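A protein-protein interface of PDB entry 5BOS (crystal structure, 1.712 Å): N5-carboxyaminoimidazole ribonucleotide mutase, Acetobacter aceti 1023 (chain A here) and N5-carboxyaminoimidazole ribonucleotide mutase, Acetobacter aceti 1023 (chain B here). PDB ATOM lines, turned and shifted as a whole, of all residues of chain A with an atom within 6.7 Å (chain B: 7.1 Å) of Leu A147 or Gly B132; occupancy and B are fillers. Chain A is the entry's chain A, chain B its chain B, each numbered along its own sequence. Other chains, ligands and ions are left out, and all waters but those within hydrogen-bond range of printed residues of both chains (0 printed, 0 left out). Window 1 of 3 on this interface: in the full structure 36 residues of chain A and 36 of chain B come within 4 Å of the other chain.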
ATOM      1  N   LEU A  44      25.586 -23.344 -27.519  1.00  0.00           N
ATOM      2  CA  LEU A  44      24.232 -23.158 -28.027  1.00  0.00           C
ATOM      3  C   LEU A  44      24.271 -22.608 -29.456  1.00  0.00           C
ATOM      4  O   LEU A  44      23.537 -23.069 -30.322  1.00  0.00           O
ATOM      5  CB  LEU A  44      23.448 -22.218 -27.103  1.00  0.00           C
ATOM      6  CG  LEU A  44      21.930 -22.075 -27.242  1.00  0.00           C
ATOM      7  CD1 LEU A  44      21.541 -21.241 -28.471  1.00  0.00           C
ATOM      8  CD2 LEU A  44      21.237 -23.434 -27.276  1.00  0.00           C
ATOM      9  N   VAL A  80      25.028  -9.227 -33.442  1.00  0.00           N
ATOM     10  CA  VAL A  80      24.776  -9.227 -32.000  1.00  0.00           C
ATOM     11  C   VAL A  80      26.083  -9.490 -31.269  1.00  0.00           C
ATOM     12  O   VAL A  80      26.890 -10.303 -31.729  1.00  0.00           O
ATOM     13  CB  VAL A  80      23.745 -10.329 -31.579  1.00  0.00           C
ATOM     14  CG1 VAL A  80      23.465 -10.276 -30.064  1.00  0.00           C
ATOM     15  CG2 VAL A  80      22.441 -10.203 -32.363  1.00  0.00           C
ATOM     16  N   LEU A 104      24.186  -7.996 -25.497  1.00  0.00           N
ATOM     17  CA  LEU A 104      23.560  -8.818 -24.466  1.00  0.00           C
ATOM     18  C   LEU A 104      24.607  -9.098 -23.409  1.00  0.00           C
ATOM     19  O   LEU A 104      25.739  -9.452 -23.733  1.00  0.00           O
ATOM     20  CB  LEU A 104      23.014 -10.118 -25.062  1.00  0.00           C
ATOM     21  CG  LEU A 104      22.115  -9.934 -26.283  1.00  0.00           C
ATOM     22  CD1 LEU A 104      21.588 -11.296 -26.787  1.00  0.00           C
ATOM     23  CD2 LEU A 104      20.958  -8.995 -25.981  1.00  0.00           C
ATOM     24  N   VAL A 131      21.927  -2.433 -22.392  1.00  0.00           N
ATOM     25  CA  VAL A 131      22.459  -3.797 -22.419  1.00  0.00           C
ATOM     26  C   VAL A 131      21.321  -4.726 -22.023  1.00  0.00           C
ATOM     27  O   VAL A 131      20.734  -4.572 -20.951  1.00  0.00           O
ATOM     28  CB  VAL A 131      23.661  -3.990 -21.465  1.00  0.00           C
ATOM     29  CG1 VAL A 131      24.040  -5.496 -21.377  1.00  0.00           C
ATOM     30  CG2 VAL A 131      24.865  -3.172 -21.948  1.00  0.00           C
ATOM     31  N   GLY A 132      20.987  -5.681 -22.884  1.00  0.00           N
ATOM     32  CA  GLY A 132      19.961  -6.645 -22.532  1.00  0.00           C
ATOM     33  C   GLY A 132      20.600  -7.698 -21.646  1.00  0.00           C
ATOM     34  O   GLY A 132      21.465  -8.442 -22.093  1.00  0.00           O
ATOM     35  N   THR A 133      20.169  -7.756 -20.387  1.00  0.00           N
ATOM     36  CA  THR A 133      20.872  -8.563 -19.386  1.00  0.00           C
ATOM     37  C   THR A 133      20.170  -9.887 -19.126  1.00  0.00           C
ATOM     38  O   THR A 133      18.949  -9.950 -19.047  1.00  0.00           O
ATOM     39  CB  THR A 133      21.012  -7.775 -18.068  1.00  0.00           C
ATOM     40  OG1 THR A 133      21.552  -6.479 -18.369  1.00  0.00           O
ATOM     41  CG2 THR A 133      21.967  -8.491 -17.090  1.00  0.00           C
ATOM     42  N   LEU A 134      20.968 -10.943 -18.996  1.00  0.00           N
ATOM     43  CA  LEU A 134      20.449 -12.277 -18.722  1.00  0.00           C
ATOM     44  C   LEU A 134      20.822 -12.703 -17.300  1.00  0.00           C
ATOM     45  O   LEU A 134      21.496 -11.958 -16.591  1.00  0.00           O
ATOM     46  CB  LEU A 134      21.001 -13.277 -19.754  1.00  0.00           C
ATOM     47  CG  LEU A 134      20.486 -13.161 -21.200  1.00  0.00           C
ATOM     48  CD1 LEU A 134      18.967 -13.150 -21.271  1.00  0.00           C
ATOM     49  CD2 LEU A 134      21.072 -11.933 -21.941  1.00  0.00           C
ATOM     50  N   LYS A 142      23.641 -19.362 -21.651  1.00  0.00           N
ATOM     51  CA  LYS A 142      22.762 -20.098 -22.560  1.00  0.00           C
ATOM     52  C   LYS A 142      21.666 -19.185 -23.102  1.00  0.00           C
ATOM     53  O   LYS A 142      21.380 -19.172 -24.301  1.00  0.00           O
ATOM     54  CB  LYS A 142      22.157 -21.308 -21.835  1.00  0.00           C
ATOM     55  CG  LYS A 142      21.237 -22.159 -22.701  1.00  0.00           C
ATOM     56  CD  LYS A 142      20.881 -23.440 -21.960  1.00  0.00           C
ATOM     57  CE  LYS A 142      19.766 -24.209 -22.663  1.00  0.00           C
ATOM     58  NZ  LYS A 142      19.435 -25.469 -21.931  1.00  0.00           N
ATOM     59  N   ASN A 143      21.054 -18.396 -22.225  1.00  0.00           N
ATOM     60  CA  ASN A 143      19.960 -17.549 -22.677  1.00  0.00           C
ATOM     61  C   ASN A 143      20.401 -16.384 -23.539  1.00  0.00           C
ATOM     62  O   ASN A 143      19.638 -15.938 -24.396  1.00  0.00           O
ATOM     63  CB  ASN A 143      19.155 -17.054 -21.481  1.00  0.00           C
ATOM     64  CG  ASN A 143      18.185 -18.097 -20.991  1.00  0.00           C
ATOM     65  OD1 ASN A 143      17.933 -19.085 -21.689  1.00  0.00           O
ATOM     66  ND2 ASN A 143      17.623 -17.892 -19.804  1.00  0.00           N
ATOM     67  N   ALA A 144      21.626 -15.894 -23.341  1.00  0.00           N
ATOM     68  CA  ALA A 144      22.118 -14.843 -24.211  1.00  0.00           C
ATOM     69  C   ALA A 144      22.240 -15.381 -25.636  1.00  0.00           C
ATOM     70  O   ALA A 144      21.876 -14.699 -26.603  1.00  0.00           O
ATOM     71  CB  ALA A 144      23.455 -14.307 -23.710  1.00  0.00           C
ATOM     72  N   ALA A 145      22.739 -16.608 -25.769  1.00  0.00           N
ATOM     73  CA  ALA A 145      22.823 -17.241 -27.085  1.00  0.00           C
ATOM     74  C   ALA A 145      21.433 -17.456 -27.695  1.00  0.00           C
ATOM     75  O   ALA A 145      21.229 -17.200 -28.879  1.00  0.00           O
ATOM     76  CB  ALA A 145      23.582 -18.567 -26.998  1.00  0.00           C
ATOM     77  N   LEU A 146      20.469 -17.903 -26.893  1.00  0.00           N
ATOM     78  CA  LEU A 146      19.106 -18.092 -27.406  1.00  0.00           C
ATOM     79  C   LEU A 146      18.449 -16.768 -27.790  1.00  0.00           C
ATOM     80  O   LEU A 146      17.743 -16.690 -28.793  1.00  0.00           O
ATOM     81  CB  LEU A 146      18.237 -18.818 -26.377  1.00  0.00           C
ATOM     82  CG  LEU A 146      18.500 -20.321 -26.292  1.00  0.00           C
ATOM     83  CD1 LEU A 146      17.986 -20.880 -24.967  1.00  0.00           C
ATOM     84  CD2 LEU A 146      17.823 -21.034 -27.455  1.00  0.00           C
ATOM     85  N   LEU A 147      18.684 -15.729 -26.992  1.00  0.00           N
ATOM     86  CA  LEU A 147      18.148 -14.413 -27.317  1.00  0.00           C
ATOM     87  C   LEU A 147      18.805 -13.892 -28.612  1.00  0.00           C
ATOM     88  O   LEU A 147      18.120 -13.355 -29.481  1.00  0.00           O
ATOM     89  CB  LEU A 147      18.354 -13.455 -26.136  1.00  0.00           C
ATOM     90  CG  LEU A 147      17.777 -12.041 -26.290  1.00  0.00           C
ATOM     91  CD1 LEU A 147      16.295 -12.074 -26.628  1.00  0.00           C
ATOM     92  CD2 LEU A 147      18.025 -11.240 -25.012  1.00  0.00           C
ATOM     93  N   ALA A 148      20.112 -14.098 -28.771  1.00  0.00           N
ATOM     94  CA  ALA A 148      20.779 -13.725 -30.025  1.00  0.00           C
ATOM     95  C   ALA A 148      20.152 -14.480 -31.193  1.00  0.00           C
ATOM     96  O   ALA A 148      19.903 -13.911 -32.258  1.00  0.00           O
ATOM     97  CB  ALA A 148      22.275 -14.008 -29.957  1.00  0.00           C
ATOM     98  N   ALA A 149      19.894 -15.765 -30.992  1.00  0.00           N
ATOM     99  CA  ALA A 149      19.253 -16.569 -32.034  1.00  0.00           C
ATOM    100  C   ALA A 149      17.868 -16.037 -32.389  1.00  0.00           C
ATOM    101  O   ALA A 149      17.499 -15.991 -33.567  1.00  0.00           O
ATOM    102  CB  ALA A 149      19.148 -18.024 -31.598  1.00  0.00           C
ATOM    103  N   SER A 150      17.095 -15.639 -31.379  1.00  0.00           N
ATOM    104  CA  SER A 150      15.741 -15.164 -31.644  1.00  0.00           C
ATOM    105  C   SER A 150      15.772 -13.828 -32.399  1.00  0.00           C
ATOM    106  O   SER A 150      14.863 -13.524 -33.171  1.00  0.00           O
ATOM    107  CB  SER A 150      14.925 -15.040 -30.340  1.00  0.00           C
ATOM    108  OG  SER A 150      15.388 -13.970 -29.535  1.00  0.00           O
ATOM    109  N   ILE A 151      16.826 -13.044 -32.184  1.00  0.00           N
ATOM    110  CA  ILE A 151      17.025 -11.806 -32.933  1.00  0.00           C
ATOM    111  C   ILE A 151      17.359 -12.117 -34.400  1.00  0.00           C
ATOM    112  O   ILE A 151      16.743 -11.573 -35.327  1.00  0.00           O
ATOM    113  CB  ILE A 151      18.136 -10.950 -32.284  1.00  0.00           C
ATOM    114  CG1 ILE A 151      17.614 -10.370 -30.965  1.00  0.00           C
ATOM    115  CG2 ILE A 151      18.569  -9.822 -33.218  1.00  0.00           C
ATOM    116  CD1 ILE A 151      18.724  -9.823 -30.056  1.00  0.00           C
ATOM    117  N   LEU A 152      18.321 -13.009 -34.610  1.00  0.00           N
ATOM    118  CA  LEU A 152      18.712 -13.365 -35.971  1.00  0.00           C
ATOM    119  C   LEU A 152      17.574 -14.047 -36.731  1.00  0.00           C
ATOM    120  O   LEU A 152      17.460 -13.899 -37.947  1.00  0.00           O
ATOM    121  CB  LEU A 152      19.946 -14.276 -35.944  1.00  0.00           C
ATOM    122  CG  LEU A 152      21.223 -13.683 -35.344  1.00  0.00           C
ATOM    123  CD1 LEU A 152      22.238 -14.791 -35.063  1.00  0.00           C
ATOM    124  CD2 LEU A 152      21.809 -12.667 -36.305  1.00  0.00           C
ATOM    125  N   ILE B  81       8.804  -7.960 -28.303  1.00  0.00           N
ATOM    126  CA  ILE B  81       7.888  -7.599 -27.225  1.00  0.00           C
ATOM    127  C   ILE B  81       8.676  -6.941 -26.098  1.00  0.00           C
ATOM    128  O   ILE B  81       9.723  -7.438 -25.679  1.00  0.00           O
ATOM    129  CB  ILE B  81       7.112  -8.830 -26.702  1.00  0.00           C
ATOM    130  CG1 ILE B  81       6.212  -9.375 -27.818  1.00  0.00           C
ATOM    131  CG2 ILE B  81       6.282  -8.448 -25.454  1.00  0.00           C
ATOM    132  CD1 ILE B  81       5.525 -10.677 -27.492  1.00  0.00           C
ATOM    133  N   ALA B  83       8.018  -5.909 -22.259  1.00  0.00           N
ATOM    134  CA  ALA B  83       7.056  -6.215 -21.199  1.00  0.00           C
ATOM    135  C   ALA B  83       7.547  -5.613 -19.894  1.00  0.00           C
ATOM    136  O   ALA B  83       8.697  -5.821 -19.515  1.00  0.00           O
ATOM    137  CB  ALA B  83       6.880  -7.754 -21.059  1.00  0.00           C
ATOM    138  N   PRO B  92       7.012 -10.639 -18.201  1.00  0.00           N
ATOM    139  CA  PRO B  92       7.986 -10.861 -19.282  1.00  0.00           C
ATOM    140  C   PRO B  92       8.348 -12.332 -19.488  1.00  0.00           C
ATOM    141  O   PRO B  92       8.428 -12.813 -20.621  1.00  0.00           O
ATOM    142  CB  PRO B  92       9.218 -10.059 -18.812  1.00  0.00           C
ATOM    143  CG  PRO B  92       8.637  -8.984 -17.919  1.00  0.00           C
ATOM    144  CD  PRO B  92       7.532  -9.703 -17.184  1.00  0.00           C
ATOM    145  N   LEU B 101       9.641 -14.961 -30.315  1.00  0.00           N
ATOM    146  CA  LEU B 101      10.202 -13.618 -30.506  1.00  0.00           C
ATOM    147  C   LEU B 101      11.105 -13.204 -29.348  1.00  0.00           C
ATOM    148  O   LEU B 101      10.933 -13.679 -28.223  1.00  0.00           O
ATOM    149  CB  LEU B 101       9.084 -12.580 -30.627  1.00  0.00           C
ATOM    150  CG  LEU B 101       8.085 -12.762 -31.765  1.00  0.00           C
ATOM    151  CD1 LEU B 101       7.005 -11.657 -31.674  1.00  0.00           C
ATOM    152  CD2 LEU B 101       8.786 -12.717 -33.116  1.00  0.00           C
ATOM    153  N   PRO B 102      12.040 -12.273 -29.598  1.00  0.00           N
ATOM    154  CA  PRO B 102      12.756 -11.725 -28.438  1.00  0.00           C
ATOM    155  C   PRO B 102      11.838 -10.926 -27.516  1.00  0.00           C
ATOM    156  O   PRO B 102      11.050 -10.102 -27.972  1.00  0.00           O
ATOM    157  CB  PRO B 102      13.823 -10.814 -29.057  1.00  0.00           C
ATOM    158  CG  PRO B 102      13.415 -10.615 -30.492  1.00  0.00           C
ATOM    159  CD  PRO B 102      12.555 -11.775 -30.887  1.00  0.00           C
ATOM    160  N   VAL B 103      11.950 -11.192 -26.223  1.00  0.00           N
ATOM    161  CA  VAL B 103      11.200 -10.467 -25.210  1.00  0.00           C
ATOM    162  C   VAL B 103      12.167  -9.697 -24.331  1.00  0.00           C
ATOM    163  O   VAL B 103      13.138 -10.276 -23.814  1.00  0.00           O
ATOM    164  CB  VAL B 103      10.371 -11.418 -24.332  1.00  0.00           C
ATOM    165  CG1 VAL B 103       9.618 -10.647 -23.258  1.00  0.00           C
ATOM    166  CG2 VAL B 103       9.424 -12.241 -25.194  1.00  0.00           C
ATOM    167  N   LEU B 104      11.899  -8.397 -24.190  1.00  0.00           N
ATOM    168  CA  LEU B 104      12.710  -7.503 -23.374  1.00  0.00           C
ATOM    169  C   LEU B 104      11.906  -7.155 -22.136  1.00  0.00           C
ATOM    170  O   LEU B 104      10.714  -6.860 -22.241  1.00  0.00           O
ATOM    171  CB  LEU B 104      13.088  -6.251 -24.167  1.00  0.00           C
ATOM    172  CG  LEU B 104      13.703  -6.533 -25.536  1.00  0.00           C
ATOM    173  CD1 LEU B 104      14.041  -5.218 -26.248  1.00  0.00           C
ATOM    174  CD2 LEU B 104      14.952  -7.406 -25.386  1.00  0.00           C
ATOM    175  N   GLY B 105      12.537  -7.227 -20.965  1.00  0.00           N
ATOM    176  CA  GLY B 105      11.809  -7.029 -19.724  1.00  0.00           C
ATOM    177  C   GLY B 105      12.233  -5.764 -19.012  1.00  0.00           C
ATOM    178  O   GLY B 105      13.421  -5.484 -18.878  1.00  0.00           O
ATOM    179  N   VAL B 106      11.253  -4.987 -18.563  1.00  0.00           N
ATOM    180  CA  VAL B 106      11.505  -3.774 -17.790  1.00  0.00           C
ATOM    181  C   VAL B 106      11.019  -3.958 -16.348  1.00  0.00           C
ATOM    182  O   VAL B 106       9.809  -4.073 -16.121  1.00  0.00           O
ATOM    183  CB  VAL B 106      10.768  -2.560 -18.387  1.00  0.00           C
ATOM    184  CG1 VAL B 106      11.002  -1.293 -17.530  1.00  0.00           C
ATOM    185  CG2 VAL B 106      11.191  -2.317 -19.842  1.00  0.00           C
ATOM    186  N   ILE B 122      12.482 -10.996 -12.973  1.00  0.00           N
ATOM    187  CA  ILE B 122      12.568 -10.913 -14.428  1.00  0.00           C
ATOM    188  C   ILE B 122      13.894 -11.454 -14.954  1.00  0.00           C
ATOM    189  O   ILE B 122      13.917 -12.251 -15.892  1.00  0.00           O
ATOM    190  CB  ILE B 122      12.371  -9.452 -14.922  1.00  0.00           C
ATOM    191  CG1 ILE B 122      10.946  -8.983 -14.590  1.00  0.00           C
ATOM    192  CG2 ILE B 122      12.669  -9.332 -16.436  1.00  0.00           C
ATOM    193  CD1 ILE B 122      10.711  -7.478 -14.832  1.00  0.00           C
ATOM    194  N   VAL B 123      15.008 -11.043 -14.355  1.00  0.00           N
ATOM    195  CA  VAL B 123      16.291 -11.349 -14.976  1.00  0.00           C
ATOM    196  C   VAL B 123      16.725 -12.806 -14.750  1.00  0.00           C
ATOM    197  O   VAL B 123      17.423 -13.383 -15.589  1.00  0.00           O
ATOM    198  CB  VAL B 123      17.403 -10.374 -14.489  1.00  0.00           C
ATOM    199  CG1 VAL B 123      17.862 -10.700 -13.059  1.00  0.00           C
ATOM    200  CG2 VAL B 123      18.605 -10.421 -15.449  1.00  0.00           C
ATOM    201  N   PRO B 130      14.720 -17.075 -22.552  1.00  0.00           N
ATOM    202  CA  PRO B 130      15.368 -15.799 -22.231  1.00  0.00           C
ATOM    203  C   PRO B 130      14.424 -14.616 -22.088  1.00  0.00           C
ATOM    204  O   PRO B 130      13.414 -14.543 -22.785  1.00  0.00           O
ATOM    205  CB  PRO B 130      16.299 -15.540 -23.435  1.00  0.00           C
ATOM    206  CG  PRO B 130      16.082 -16.666 -24.399  1.00  0.00           C
ATOM    207  CD  PRO B 130      14.870 -17.461 -23.966  1.00  0.00           C
ATOM    208  N   VAL B 131      14.793 -13.693 -21.206  1.00  0.00           N
ATOM    209  CA  VAL B 131      14.255 -12.337 -21.224  1.00  0.00           C
ATOM    210  C   VAL B 131      15.431 -11.369 -21.123  1.00  0.00           C
ATOM    211  O   VAL B 131      16.220 -11.431 -20.177  1.00  0.00           O
ATOM    212  CB  VAL B 131      13.269 -12.065 -20.070  1.00  0.00           C
ATOM    213  CG1 VAL B 131      12.916 -10.572 -20.022  1.00  0.00           C
ATOM    214  CG2 VAL B 131      12.003 -12.915 -20.230  1.00  0.00           C
ATOM    215  N   GLY B 132      15.575 -10.490 -22.107  1.00  0.00           N
ATOM    216  CA  GLY B 132      16.644  -9.507 -22.068  1.00  0.00           C
ATOM    217  C   GLY B 132      16.196  -8.388 -21.151  1.00  0.00           C
ATOM    218  O   GLY B 132      15.231  -7.689 -21.460  1.00  0.00           O
ATOM    219  N   THR B 133      16.892  -8.231 -20.029  1.00  0.00           N
ATOM    220  CA  THR B 133      16.390  -7.353 -18.963  1.00  0.00           C
ATOM    221  C   THR B 133      17.122  -6.030 -18.946  1.00  0.00           C
ATOM    222  O   THR B 133      18.330  -5.978 -19.134  1.00  0.00           O
ATOM    223  CB  THR B 133      16.516  -8.053 -17.603  1.00  0.00           C
ATOM    224  OG1 THR B 133      15.901  -9.345 -17.710  1.00  0.00           O
ATOM    225  CG2 THR B 133      15.814  -7.249 -16.499  1.00  0.00           C
ATOM    226  N   LEU B 134      16.363  -4.958 -18.723  1.00  0.00           N
ATOM    227  CA  LEU B 134      16.915  -3.610 -18.654  1.00  0.00           C
ATOM    228  C   LEU B 134      16.841  -3.087 -17.213  1.00  0.00           C
ATOM    229  O   LEU B 134      16.356  -3.791 -16.318  1.00  0.00           O
ATOM    230  CB  LEU B 134      16.165  -2.673 -19.617  1.00  0.00           C
ATOM    231  CG  LEU B 134      16.316  -2.892 -21.132  1.00  0.00           C
ATOM    232  CD1 LEU B 134      17.787  -2.937 -21.520  1.00  0.00           C
ATOM    233  CD2 LEU B 134      15.590  -4.147 -21.640  1.00  0.00           C
ATOM    234  N   ALA B 144      14.767  -0.315 -23.234  1.00  0.00           N
ATOM    235  CA  ALA B 144      14.108  -1.446 -23.889  1.00  0.00           C
ATOM    236  C   ALA B 144      13.697  -1.043 -25.302  1.00  0.00           C
ATOM    237  O   ALA B 144      13.849  -1.823 -26.255  1.00  0.00           O
ATOM    238  CB  ALA B 144      12.884  -1.921 -23.092  1.00  0.00           C
ATOM    239  N   LEU B 147      16.869  -0.815 -27.364  1.00  0.00           N
ATOM    240  CA  LEU B 147      17.352  -2.159 -27.689  1.00  0.00           C
ATOM    241  C   LEU B 147      16.472  -2.763 -28.784  1.00  0.00           C
ATOM    242  O   LEU B 147      16.982  -3.360 -29.733  1.00  0.00           O
ATOM    243  CB  LEU B 147      17.370  -3.049 -26.435  1.00  0.00           C
ATOM    244  CG  LEU B 147      17.889  -4.486 -26.609  1.00  0.00           C
ATOM    245  CD1 LEU B 147      19.258  -4.485 -27.282  1.00  0.00           C
ATOM    246  CD2 LEU B 147      17.978  -5.171 -25.244  1.00  0.00           C
ATOM    247  N   ILE B 151      17.648  -3.928 -32.623  1.00  0.00           N
ATOM    248  CA  ILE B 151      17.309  -5.227 -33.205  1.00  0.00           C
ATOM    249  C   ILE B 151      16.666  -5.020 -34.587  1.00  0.00           C
ATOM    250  O   ILE B 151      17.077  -5.629 -35.573  1.00  0.00           O
ATOM    251  CB  ILE B 151      16.351  -6.004 -32.275  1.00  0.00           C
ATOM    252  CG1 ILE B 151      17.121  -6.453 -31.026  1.00  0.00           C
ATOM    253  CG2 ILE B 151      15.688  -7.167 -33.027  1.00  0.00           C
ATOM    254  CD1 ILE B 151      16.241  -6.993 -29.924  1.00  0.00           C
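O of Thr B133 sits close to O of Val A131, 3.3 Å away. The backbone carbonyl oxygen (O) of Thr A133 sits close to the backbone carbonyl oxygen (O) of Val B131. N of Thr A133 sits at hydrogen-bond distance from O of Thr B133 (2.8 Å).
The backbone NH of Leu B134 lies within hydrogen-bond range of the backbone carbonyl oxygen of Gly B105 (3.0 Å). The backbone NH of Gly B105 lies within hydrogen-bond range of the backbone carbonyl oxygen of Gly B132. O of Leu A147 is in hydrogen-bond range of OG of Ser A150 (2.8 Å). The backbone NH (N) of Ile B81 sits at hydrogen-bond distance from the backbone carbonyl oxygen (O) of Pro B102. The backbone carbonyl oxygen of Val A131 sits at hydrogen-bond distance from the side-chain hydroxyl of Thr A133, 3.3 Å away. O of Val B131 is in hydrogen-bond range of OG1 of Thr B133, at 3.2 Å.
Among the printed residues, merely in contact across the chains: Val A131 with Leu B134 (3.4 Å), Gly A132 with Thr B133 (3.8 Å), Gly A132 with Leu B147 (3.7 Å), Thr A133 with Val B123 (3.6 Å), Thr A133 with Gly B132 (3.8 Å), Leu A134 with Val B123 (3.5 Å), Leu A134 with Val B131 (3.4 Å), Asn A143 with Pro B130 (3.5 Å), Leu A146 with Pro B130 (3.6 Å), Leu A147 with Pro B102 (3.7 Å), Leu A147 with Pro B130 (3.8 Å), Leu A147 with Gly B132 (3.7 Å), Ser A150 with Pro B102 (3.6 Å) and Ile A151 with Ile B151 (3.8 Å).
Printed residues of chain B that touch a printed residue of chain A: Pro B102, Val B123, Pro B130, Val B131, Gly B132, Thr B133, Leu B134, Leu B147 and Ile B151.
Leu A147 touches three residues of chain B. Gly B132 touches two residues of chain A. Printed residues of chain A within 4 Å of Pro B102: Leu A147 (3.7 Å) and Ser A150 (3.6 Å). Of the printed residues of chain B, Asn A143 touches Pro B130 (3.5 Å). Of the printed residues of chain A, Val B123 touches Thr A133 (3.6 Å) and Leu A134 (3.5 Å). Ala A149 touches none of the printed residues of chain B. Ala B144 touches none of the printed residues of chain A.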
